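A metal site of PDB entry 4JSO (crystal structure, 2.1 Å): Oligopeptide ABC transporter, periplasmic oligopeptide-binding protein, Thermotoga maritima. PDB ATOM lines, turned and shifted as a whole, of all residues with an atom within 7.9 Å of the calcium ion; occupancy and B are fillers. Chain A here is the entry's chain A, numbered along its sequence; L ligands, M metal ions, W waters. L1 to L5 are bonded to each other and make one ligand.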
ATOM      1  N   LEU A  23     -22.013 -22.182  34.142  1.00  0.00           N
ATOM      2  CA  LEU A  23     -21.366 -21.580  32.984  1.00  0.00           C
ATOM      3  C   LEU A  23     -21.764 -20.114  32.767  1.00  0.00           C
ATOM      4  O   LEU A  23     -21.354 -19.495  31.782  1.00  0.00           O
ATOM      5  CB  LEU A  23     -21.644 -22.397  31.719  1.00  0.00           C
ATOM      6  CG  LEU A  23     -21.161 -23.844  31.733  1.00  0.00           C
ATOM      7  CD1 LEU A  23     -21.585 -24.568  30.469  1.00  0.00           C
ATOM      8  CD2 LEU A  23     -19.639 -23.917  31.914  1.00  0.00           C
ATOM      9  N   GLY A  31     -14.521 -29.522  34.269  1.00  0.00           N
ATOM     10  CA  GLY A  31     -15.444 -30.635  34.213  1.00  0.00           C
ATOM     11  C   GLY A  31     -16.861 -30.209  33.906  1.00  0.00           C
ATOM     12  O   GLY A  31     -17.654 -31.005  33.413  1.00  0.00           O
ATOM     13  N   THR A  32     -17.184 -28.947  34.201  1.00  0.00           N
ATOM     14  CA  THR A  32     -18.535 -28.432  33.988  1.00  0.00           C
ATOM     15  C   THR A  32     -18.902 -28.394  32.505  1.00  0.00           C
ATOM     16  O   THR A  32     -19.831 -29.067  32.077  1.00  0.00           O
ATOM     17  CB  THR A  32     -18.730 -27.027  34.616  1.00  0.00           C
ATOM     18  OG1 THR A  32     -18.385 -27.061  36.010  1.00  0.00           O
ATOM     19  CG2 THR A  32     -20.175 -26.569  34.468  1.00  0.00           C
ATOM     20  N   ASP A  33     -18.188 -27.600  31.732  1.00  0.00           N
ATOM     21  CA  ASP A  33     -18.477 -27.497  30.308  1.00  0.00           C
ATOM     22  C   ASP A  33     -18.080 -28.797  29.609  1.00  0.00           C
ATOM     23  O   ASP A  33     -18.782 -29.275  28.710  1.00  0.00           O
ATOM     24  CB  ASP A  33     -17.734 -26.309  29.682  1.00  0.00           C
ATOM     25  CG  ASP A  33     -18.418 -25.772  28.435  1.00  0.00           C
ATOM     26  OD1 ASP A  33     -19.269 -26.476  27.858  1.00  0.00           O
ATOM     27  OD2 ASP A  33     -18.099 -24.627  28.029  1.00  0.00           O
ATOM     28  N   GLN A  34     -16.980 -29.396  30.050  1.00  0.00           N
ATOM     29  CA  GLN A  34     -16.458 -30.596  29.404  1.00  0.00           C
ATOM     30  C   GLN A  34     -17.391 -31.805  29.495  1.00  0.00           C
ATOM     31  O   GLN A  34     -17.643 -32.470  28.478  1.00  0.00           O
ATOM     32  CB  GLN A  34     -15.069 -30.962  29.945  1.00  0.00           C
ATOM     33  CG  GLN A  34     -13.967 -29.982  29.587  1.00  0.00           C
ATOM     34  CD  GLN A  34     -13.783 -28.875  30.609  1.00  0.00           C
ATOM     35  OE1 GLN A  34     -14.572 -28.745  31.540  1.00  0.00           O
ATOM     36  NE2 GLN A  34     -12.735 -28.074  30.445  1.00  0.00           N
ATOM     37  N   PHE A  35     -17.907 -32.091  30.692  1.00  0.00           N
ATOM     38  CA  PHE A  35     -18.635 -33.343  30.931  1.00  0.00           C
ATOM     39  C   PHE A  35     -20.120 -33.173  31.324  1.00  0.00           C
ATOM     40  O   PHE A  35     -20.930 -34.077  31.097  1.00  0.00           O
ATOM     41  CB  PHE A  35     -17.906 -34.181  31.983  1.00  0.00           C
ATOM     42  CG  PHE A  35     -16.410 -34.308  31.760  1.00  0.00           C
ATOM     43  CD1 PHE A  35     -15.892 -34.698  30.530  1.00  0.00           C
ATOM     44  CD2 PHE A  35     -15.521 -34.046  32.799  1.00  0.00           C
ATOM     45  CE1 PHE A  35     -14.496 -34.815  30.332  1.00  0.00           C
ATOM     46  CE2 PHE A  35     -14.135 -34.156  32.613  1.00  0.00           C
ATOM     47  CZ  PHE A  35     -13.618 -34.536  31.385  1.00  0.00           C
ATOM     48  N   MET A  36     -20.490 -32.031  31.884  1.00  0.00           N
ATOM     49  CA  MET A  36     -21.863 -31.857  32.355  1.00  0.00           C
ATOM     50  C   MET A  36     -22.829 -31.387  31.289  1.00  0.00           C
ATOM     51  O   MET A  36     -24.019 -31.736  31.311  1.00  0.00           O
ATOM     52  CB  MET A  36     -21.905 -30.918  33.570  1.00  0.00           C
ATOM     53  CG  MET A  36     -21.287 -31.521  34.817  1.00  0.00           C
ATOM     54  SD  MET A  36     -21.102 -30.334  36.147  1.00  0.00           S
ATOM     55  CE  MET A  36     -22.721 -29.595  36.194  1.00  0.00           C
ATOM     56  N   TYR A  37     -22.340 -30.589  30.352  1.00  0.00           N
ATOM     57  CA  TYR A  37     -23.191 -30.016  29.320  1.00  0.00           C
ATOM     58  C   TYR A  37     -22.673 -30.315  27.913  1.00  0.00           C
ATOM     59  O   TYR A  37     -21.564 -29.914  27.558  1.00  0.00           O
ATOM     60  CB  TYR A  37     -23.342 -28.508  29.539  1.00  0.00           C
ATOM     61  CG  TYR A  37     -23.854 -28.154  30.924  1.00  0.00           C
ATOM     62  CD1 TYR A  37     -25.203 -28.259  31.246  1.00  0.00           C
ATOM     63  CD2 TYR A  37     -22.977 -27.710  31.903  1.00  0.00           C
ATOM     64  CE1 TYR A  37     -25.666 -27.933  32.514  1.00  0.00           C
ATOM     65  CE2 TYR A  37     -23.430 -27.384  33.171  1.00  0.00           C
ATOM     66  CZ  TYR A  37     -24.770 -27.494  33.471  1.00  0.00           C
ATOM     67  OH  TYR A  37     -25.192 -27.166  34.737  1.00  0.00           O
ATOM     68  N   LEU A  38     -23.467 -31.031  27.129  1.00  0.00           N
ATOM     69  CA  LEU A  38     -23.081 -31.448  25.778  1.00  0.00           C
ATOM     70  C   LEU A  38     -23.703 -30.558  24.690  1.00  0.00           C
ATOM     71  O   LEU A  38     -24.655 -29.828  24.967  1.00  0.00           O
ATOM     72  CB  LEU A  38     -23.454 -32.916  25.553  1.00  0.00           C
ATOM     73  CG  LEU A  38     -22.750 -33.879  26.504  1.00  0.00           C
ATOM     74  CD1 LEU A  38     -23.216 -35.318  26.257  1.00  0.00           C
ATOM     75  CD2 LEU A  38     -21.228 -33.755  26.362  1.00  0.00           C
ATOM     76  N   PRO A  39     -23.167 -30.601  23.458  1.00  0.00           N
ATOM     77  CA  PRO A  39     -23.706 -29.742  22.403  1.00  0.00           C
ATOM     78  C   PRO A  39     -24.712 -30.484  21.520  1.00  0.00           C
ATOM     79  O   PRO A  39     -24.883 -31.696  21.656  1.00  0.00           O
ATOM     80  CB  PRO A  39     -22.462 -29.426  21.583  1.00  0.00           C
ATOM     81  CG  PRO A  39     -21.678 -30.711  21.644  1.00  0.00           C
ATOM     82  CD  PRO A  39     -21.941 -31.296  23.016  1.00  0.00           C
ATOM     83  N   GLN A  42     -21.097 -32.425  18.191  1.00  0.00           N
ATOM     84  CA  GLN A  42     -19.730 -32.314  18.671  1.00  0.00           C
ATOM     85  C   GLN A  42     -18.763 -32.332  17.500  1.00  0.00           C
ATOM     86  O   GLN A  42     -18.687 -33.321  16.772  1.00  0.00           O
ATOM     87  CB  GLN A  42     -19.405 -33.473  19.622  1.00  0.00           C
ATOM     88  CG  GLN A  42     -17.910 -33.512  20.012  1.00  0.00           C
ATOM     89  CD  GLN A  42     -17.518 -32.286  20.824  1.00  0.00           C
ATOM     90  OE1 GLN A  42     -18.049 -32.055  21.906  1.00  0.00           O
ATOM     91  NE2 GLN A  42     -16.598 -31.490  20.289  1.00  0.00           N
ATOM     92  N   PRO A 101     -22.194 -19.614  27.600  1.00  0.00           N
ATOM     93  CA  PRO A 101     -21.882 -20.386  26.394  1.00  0.00           C
ATOM     94  C   PRO A 101     -22.528 -19.813  25.132  1.00  0.00           C
ATOM     95  O   PRO A 101     -23.696 -19.407  25.148  1.00  0.00           O
ATOM     96  CB  PRO A 101     -22.458 -21.776  26.717  1.00  0.00           C
ATOM     97  CG  PRO A 101     -23.492 -21.528  27.767  1.00  0.00           C
ATOM     98  CD  PRO A 101     -22.964 -20.396  28.580  1.00  0.00           C
ATOM     99  N   GLY A 140     -22.935 -26.273  17.046  1.00  0.00           N
ATOM    100  CA  GLY A 140     -22.306 -26.396  18.344  1.00  0.00           C
ATOM    101  C   GLY A 140     -23.123 -25.893  19.521  1.00  0.00           C
ATOM    102  O   GLY A 140     -22.644 -25.924  20.647  1.00  0.00           O
ATOM    103  N   GLN A 142     -25.145 -25.243  22.752  1.00  0.00           N
ATOM    104  CA  GLN A 142     -25.311 -25.982  23.993  1.00  0.00           C
ATOM    105  C   GLN A 142     -26.585 -25.558  24.695  1.00  0.00           C
ATOM    106  O   GLN A 142     -26.706 -24.422  25.145  1.00  0.00           O
ATOM    107  CB  GLN A 142     -24.154 -25.710  24.944  1.00  0.00           C
ATOM    108  CG  GLN A 142     -22.857 -26.383  24.574  1.00  0.00           C
ATOM    109  CD  GLN A 142     -21.982 -26.630  25.792  1.00  0.00           C
ATOM    110  OE1 GLN A 142     -21.555 -27.742  26.027  1.00  0.00           O
ATOM    111  NE2 GLN A 142     -21.750 -25.582  26.580  1.00  0.00           N
ATOM    112  N   SER A 172     -26.769 -32.616  30.929  1.00  0.00           N
ATOM    113  CA  SER A 172     -27.033 -33.324  29.683  1.00  0.00           C
ATOM    114  C   SER A 172     -25.952 -34.365  29.370  1.00  0.00           C
ATOM    115  O   SER A 172     -26.136 -35.238  28.529  1.00  0.00           O
ATOM    116  CB  SER A 172     -27.162 -32.331  28.525  1.00  0.00           C
ATOM    117  OG  SER A 172     -26.088 -31.414  28.522  1.00  0.00           O
ATOM    118  N   HIS A 536      -9.271 -30.244  27.752  1.00  0.00           N
ATOM    119  CA  HIS A 536      -9.804 -29.709  26.511  1.00  0.00           C
ATOM    120  C   HIS A 536     -11.333 -29.624  26.495  1.00  0.00           C
ATOM    121  O   HIS A 536     -12.008 -30.480  27.053  1.00  0.00           O
ATOM    122  CB  HIS A 536      -9.330 -30.510  25.294  1.00  0.00           C
ATOM    123  CG  HIS A 536      -9.447 -29.760  24.014  1.00  0.00           C
ATOM    124  ND1 HIS A 536     -10.608 -29.732  23.266  1.00  0.00           N
ATOM    125  CD2 HIS A 536      -8.570 -28.964  23.348  1.00  0.00           C
ATOM    126  CE1 HIS A 536     -10.439 -28.981  22.200  1.00  0.00           C
ATOM    127  NE2 HIS A 536      -9.206 -28.496  22.230  1.00  0.00           N
ATOM    128  N   ALA A 537     -11.864 -28.591  25.854  1.00  0.00           N
ATOM    129  CA  ALA A 537     -13.311 -28.412  25.730  1.00  0.00           C
ATOM    130  C   ALA A 537     -14.010 -29.628  25.112  1.00  0.00           C
ATOM    131  O   ALA A 537     -15.194 -29.849  25.338  1.00  0.00           O
ATOM    132  CB  ALA A 537     -13.630 -27.138  24.941  1.00  0.00           C
ATOM    133  N   ASP A 538     -13.257 -30.407  24.337  1.00  0.00           N
ATOM    134  CA  ASP A 538     -13.835 -31.521  23.580  1.00  0.00           C
ATOM    135  C   ASP A 538     -13.279 -32.894  23.959  1.00  0.00           C
ATOM    136  O   ASP A 538     -13.192 -33.782  23.117  1.00  0.00           O
ATOM    137  CB  ASP A 538     -13.613 -31.293  22.079  1.00  0.00           C
ATOM    138  CG  ASP A 538     -14.169 -29.956  21.612  1.00  0.00           C
ATOM    139  OD1 ASP A 538     -15.314 -29.622  22.001  1.00  0.00           O
ATOM    140  OD2 ASP A 538     -13.449 -29.249  20.876  1.00  0.00           O
ATOM    141  N   TRP A 540     -14.488 -35.228  26.021  1.00  0.00           N
ATOM    142  CA  TRP A 540     -15.414 -36.243  26.530  1.00  0.00           C
ATOM    143  C   TRP A 540     -15.421 -37.643  25.858  1.00  0.00           C
ATOM    144  O   TRP A 540     -15.573 -38.645  26.557  1.00  0.00           O
ATOM    145  CB  TRP A 540     -16.839 -35.677  26.704  1.00  0.00           C
ATOM    146  CG  TRP A 540     -17.548 -35.391  25.436  1.00  0.00           C
ATOM    147  CD1 TRP A 540     -17.648 -34.189  24.790  1.00  0.00           C
ATOM    148  CD2 TRP A 540     -18.278 -36.333  24.632  1.00  0.00           C
ATOM    149  NE1 TRP A 540     -18.388 -34.321  23.636  1.00  0.00           N
ATOM    150  CE2 TRP A 540     -18.779 -35.635  23.519  1.00  0.00           C
ATOM    151  CE3 TRP A 540     -18.550 -37.692  24.757  1.00  0.00           C
ATOM    152  CZ2 TRP A 540     -19.543 -36.255  22.537  1.00  0.00           C
ATOM    153  CZ3 TRP A 540     -19.305 -38.311  23.775  1.00  0.00           C
ATOM    154  CH2 TRP A 540     -19.796 -37.595  22.684  1.00  0.00           C
HETATM  155  C1  LIG L   1     -15.853 -20.270  29.601  1.00  0.00           C
HETATM  156  C2  LIG L   1     -15.782 -20.873  31.019  1.00  0.00           C
HETATM  157  C3  LIG L   1     -16.651 -20.105  31.990  1.00  0.00           C
HETATM  158  C4  LIG L   1     -18.062 -19.844  31.462  1.00  0.00           C
HETATM  159  C5  LIG L   1     -18.491 -18.629  32.289  1.00  0.00           C
HETATM  160  C6  LIG L   1     -17.316 -20.275  29.122  1.00  0.00           C
HETATM  161  O1  LIG L   1     -17.351 -19.532  27.909  1.00  0.00           O
HETATM  162  O2  LIG L   1     -15.027 -20.984  28.652  1.00  0.00           O
HETATM  163  O3  LIG L   1     -14.454 -20.905  31.609  1.00  0.00           O
HETATM  164  O4  LIG L   1     -16.729 -20.807  33.223  1.00  0.00           O
HETATM  165  O5  LIG L   1     -18.210 -19.600  30.036  1.00  0.00           O
HETATM  166  O6  LIG L   1     -18.901 -19.129  33.589  1.00  0.00           O
HETATM  167  C1  LG2 L   2     -12.599 -22.268  31.845  1.00  0.00           C
HETATM  168  C2  LG2 L   2     -12.172 -23.708  31.619  1.00  0.00           C
HETATM  169  C3  LG2 L   2     -12.960 -24.744  32.414  1.00  0.00           C
HETATM  170  C4  LG2 L   2     -14.433 -24.525  32.165  1.00  0.00           C
HETATM  171  C5  LG2 L   2     -15.303 -25.587  32.847  1.00  0.00           C
HETATM  172  C6  LG2 L   2     -14.068 -22.260  31.581  1.00  0.00           C
HETATM  173  O1  LG2 L   2     -11.963 -21.408  30.893  1.00  0.00           O
HETATM  174  O2  LG2 L   2     -10.818 -23.749  31.972  1.00  0.00           O
HETATM  175  O3  LG2 L   2     -12.507 -26.042  32.018  1.00  0.00           O
HETATM  176  O4  LG2 L   2     -14.752 -23.159  32.507  1.00  0.00           O
HETATM  177  O5  LG2 L   2     -16.635 -25.165  32.709  1.00  0.00           O
HETATM  178  C1  LG3 L   3      -8.763 -24.462  31.327  1.00  0.00           C
HETATM  179  C2  LG3 L   3      -7.828 -24.617  30.174  1.00  0.00           C
HETATM  180  C3  LG3 L   3      -8.630 -25.192  28.978  1.00  0.00           C
HETATM  181  C4  LG3 L   3      -9.833 -24.371  28.628  1.00  0.00           C
HETATM  182  C5  LG3 L   3     -10.578 -25.045  27.495  1.00  0.00           C
HETATM  183  C6  LG3 L   3     -10.012 -23.760  30.827  1.00  0.00           C
HETATM  184  O1  LG3 L   3      -8.158 -23.662  32.385  1.00  0.00           O
HETATM  185  O2  LG3 L   3      -6.799 -25.512  30.598  1.00  0.00           O
HETATM  186  O3  LG3 L   3      -7.838 -25.293  27.818  1.00  0.00           O
HETATM  187  O4  LG3 L   3     -10.666 -24.417  29.744  1.00  0.00           O
HETATM  188  O5  LG3 L   3     -11.421 -24.142  26.853  1.00  0.00           O
HETATM  189  C1  LG4 L   4      -4.646 -26.150  30.976  1.00  0.00           C
HETATM  190  C2  LG4 L   4      -3.220 -25.833  30.627  1.00  0.00           C
HETATM  191  C3  LG4 L   4      -3.067 -25.627  29.114  1.00  0.00           C
HETATM  192  C4  LG4 L   4      -3.930 -24.512  28.651  1.00  0.00           C
HETATM  193  C5  LG4 L   4      -4.131 -24.246  27.140  1.00  0.00           C
HETATM  194  C6  LG4 L   4      -5.480 -25.031  30.442  1.00  0.00           C
HETATM  195  O1  LG4 L   4      -4.860 -26.379  32.365  1.00  0.00           O
HETATM  196  O2  LG4 L   4      -2.459 -26.919  31.119  1.00  0.00           O
HETATM  197  O3  LG4 L   4      -1.693 -25.240  28.931  1.00  0.00           O
HETATM  198  O4  LG4 L   4      -5.241 -24.865  29.072  1.00  0.00           O
HETATM  199  O5  LG4 L   4      -2.856 -23.823  26.651  1.00  0.00           O
HETATM  200  C1  LG5 L   5      -0.643 -27.710  32.518  1.00  0.00           C
HETATM  201  C2  LG5 L   5       0.564 -27.315  33.366  1.00  0.00           C
HETATM  202  C3  LG5 L   5       1.462 -26.455  32.507  1.00  0.00           C
HETATM  203  C4  LG5 L   5       0.706 -25.374  31.801  1.00  0.00           C
HETATM  204  C5  LG5 L   5       1.504 -24.580  30.762  1.00  0.00           C
HETATM  205  C6  LG5 L   5      -1.336 -26.495  31.883  1.00  0.00           C
HETATM  206  O1  LG5 L   5      -1.482 -28.382  33.427  1.00  0.00           O
HETATM  207  O2  LG5 L   5       1.327 -28.458  33.777  1.00  0.00           O
HETATM  208  O3  LG5 L   5       2.572 -25.854  33.180  1.00  0.00           O
HETATM  209  O4  LG5 L   5      -0.412 -25.867  31.086  1.00  0.00           O
HETATM  210  O5  LG5 L   5       2.185 -25.386  29.822  1.00  0.00           O
HETATM  211 CA    CA M   1     -19.657 -28.659  26.762  1.00  0.00          CA
HETATM  212  O   HOH W   1     -17.175 -27.892  26.525  1.00  0.00           O
HETATM  213  O   HOH W   2     -18.883 -30.834  26.076  1.00  0.00           O
HETATM  214  O   HOH W   3     -19.723 -28.749  24.467  1.00  0.00           O
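N of Tyr 37 is in hydrogen-bond range of O of Thr 32 (3.4 Å).
The backbone NH (N) of Asp 33 sits at hydrogen-bond distance from an oxygen (O5) of LG2 L2, 3.0 Å away.
An oxygen (O3) of LG2 L2 is in hydrogen-bond range of the side-chain amide nitrogen (NE2) of Gln 34, 2.6 Å away.
O6 of LIG L1 sits close to O of Leu 23 (3.1 Å).
The calcium ion is bound by the backbone carbonyl oxygen of Asp 33 (2.2 Å), the side-chain amide oxygen of Gln 142 (2.2 Å), water W3 (2.3 Å), water W2 (2.4 Å), the backbone carbonyl oxygen of Tyr 37 (2.4 Å), the side-chain carboxylate of Asp 33 (2.5 Å) and water W1 (2.6 Å).
Three residues have an atom within 4 Å of the calcium ion: Asp 33, Tyr 37 and Gln 142.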
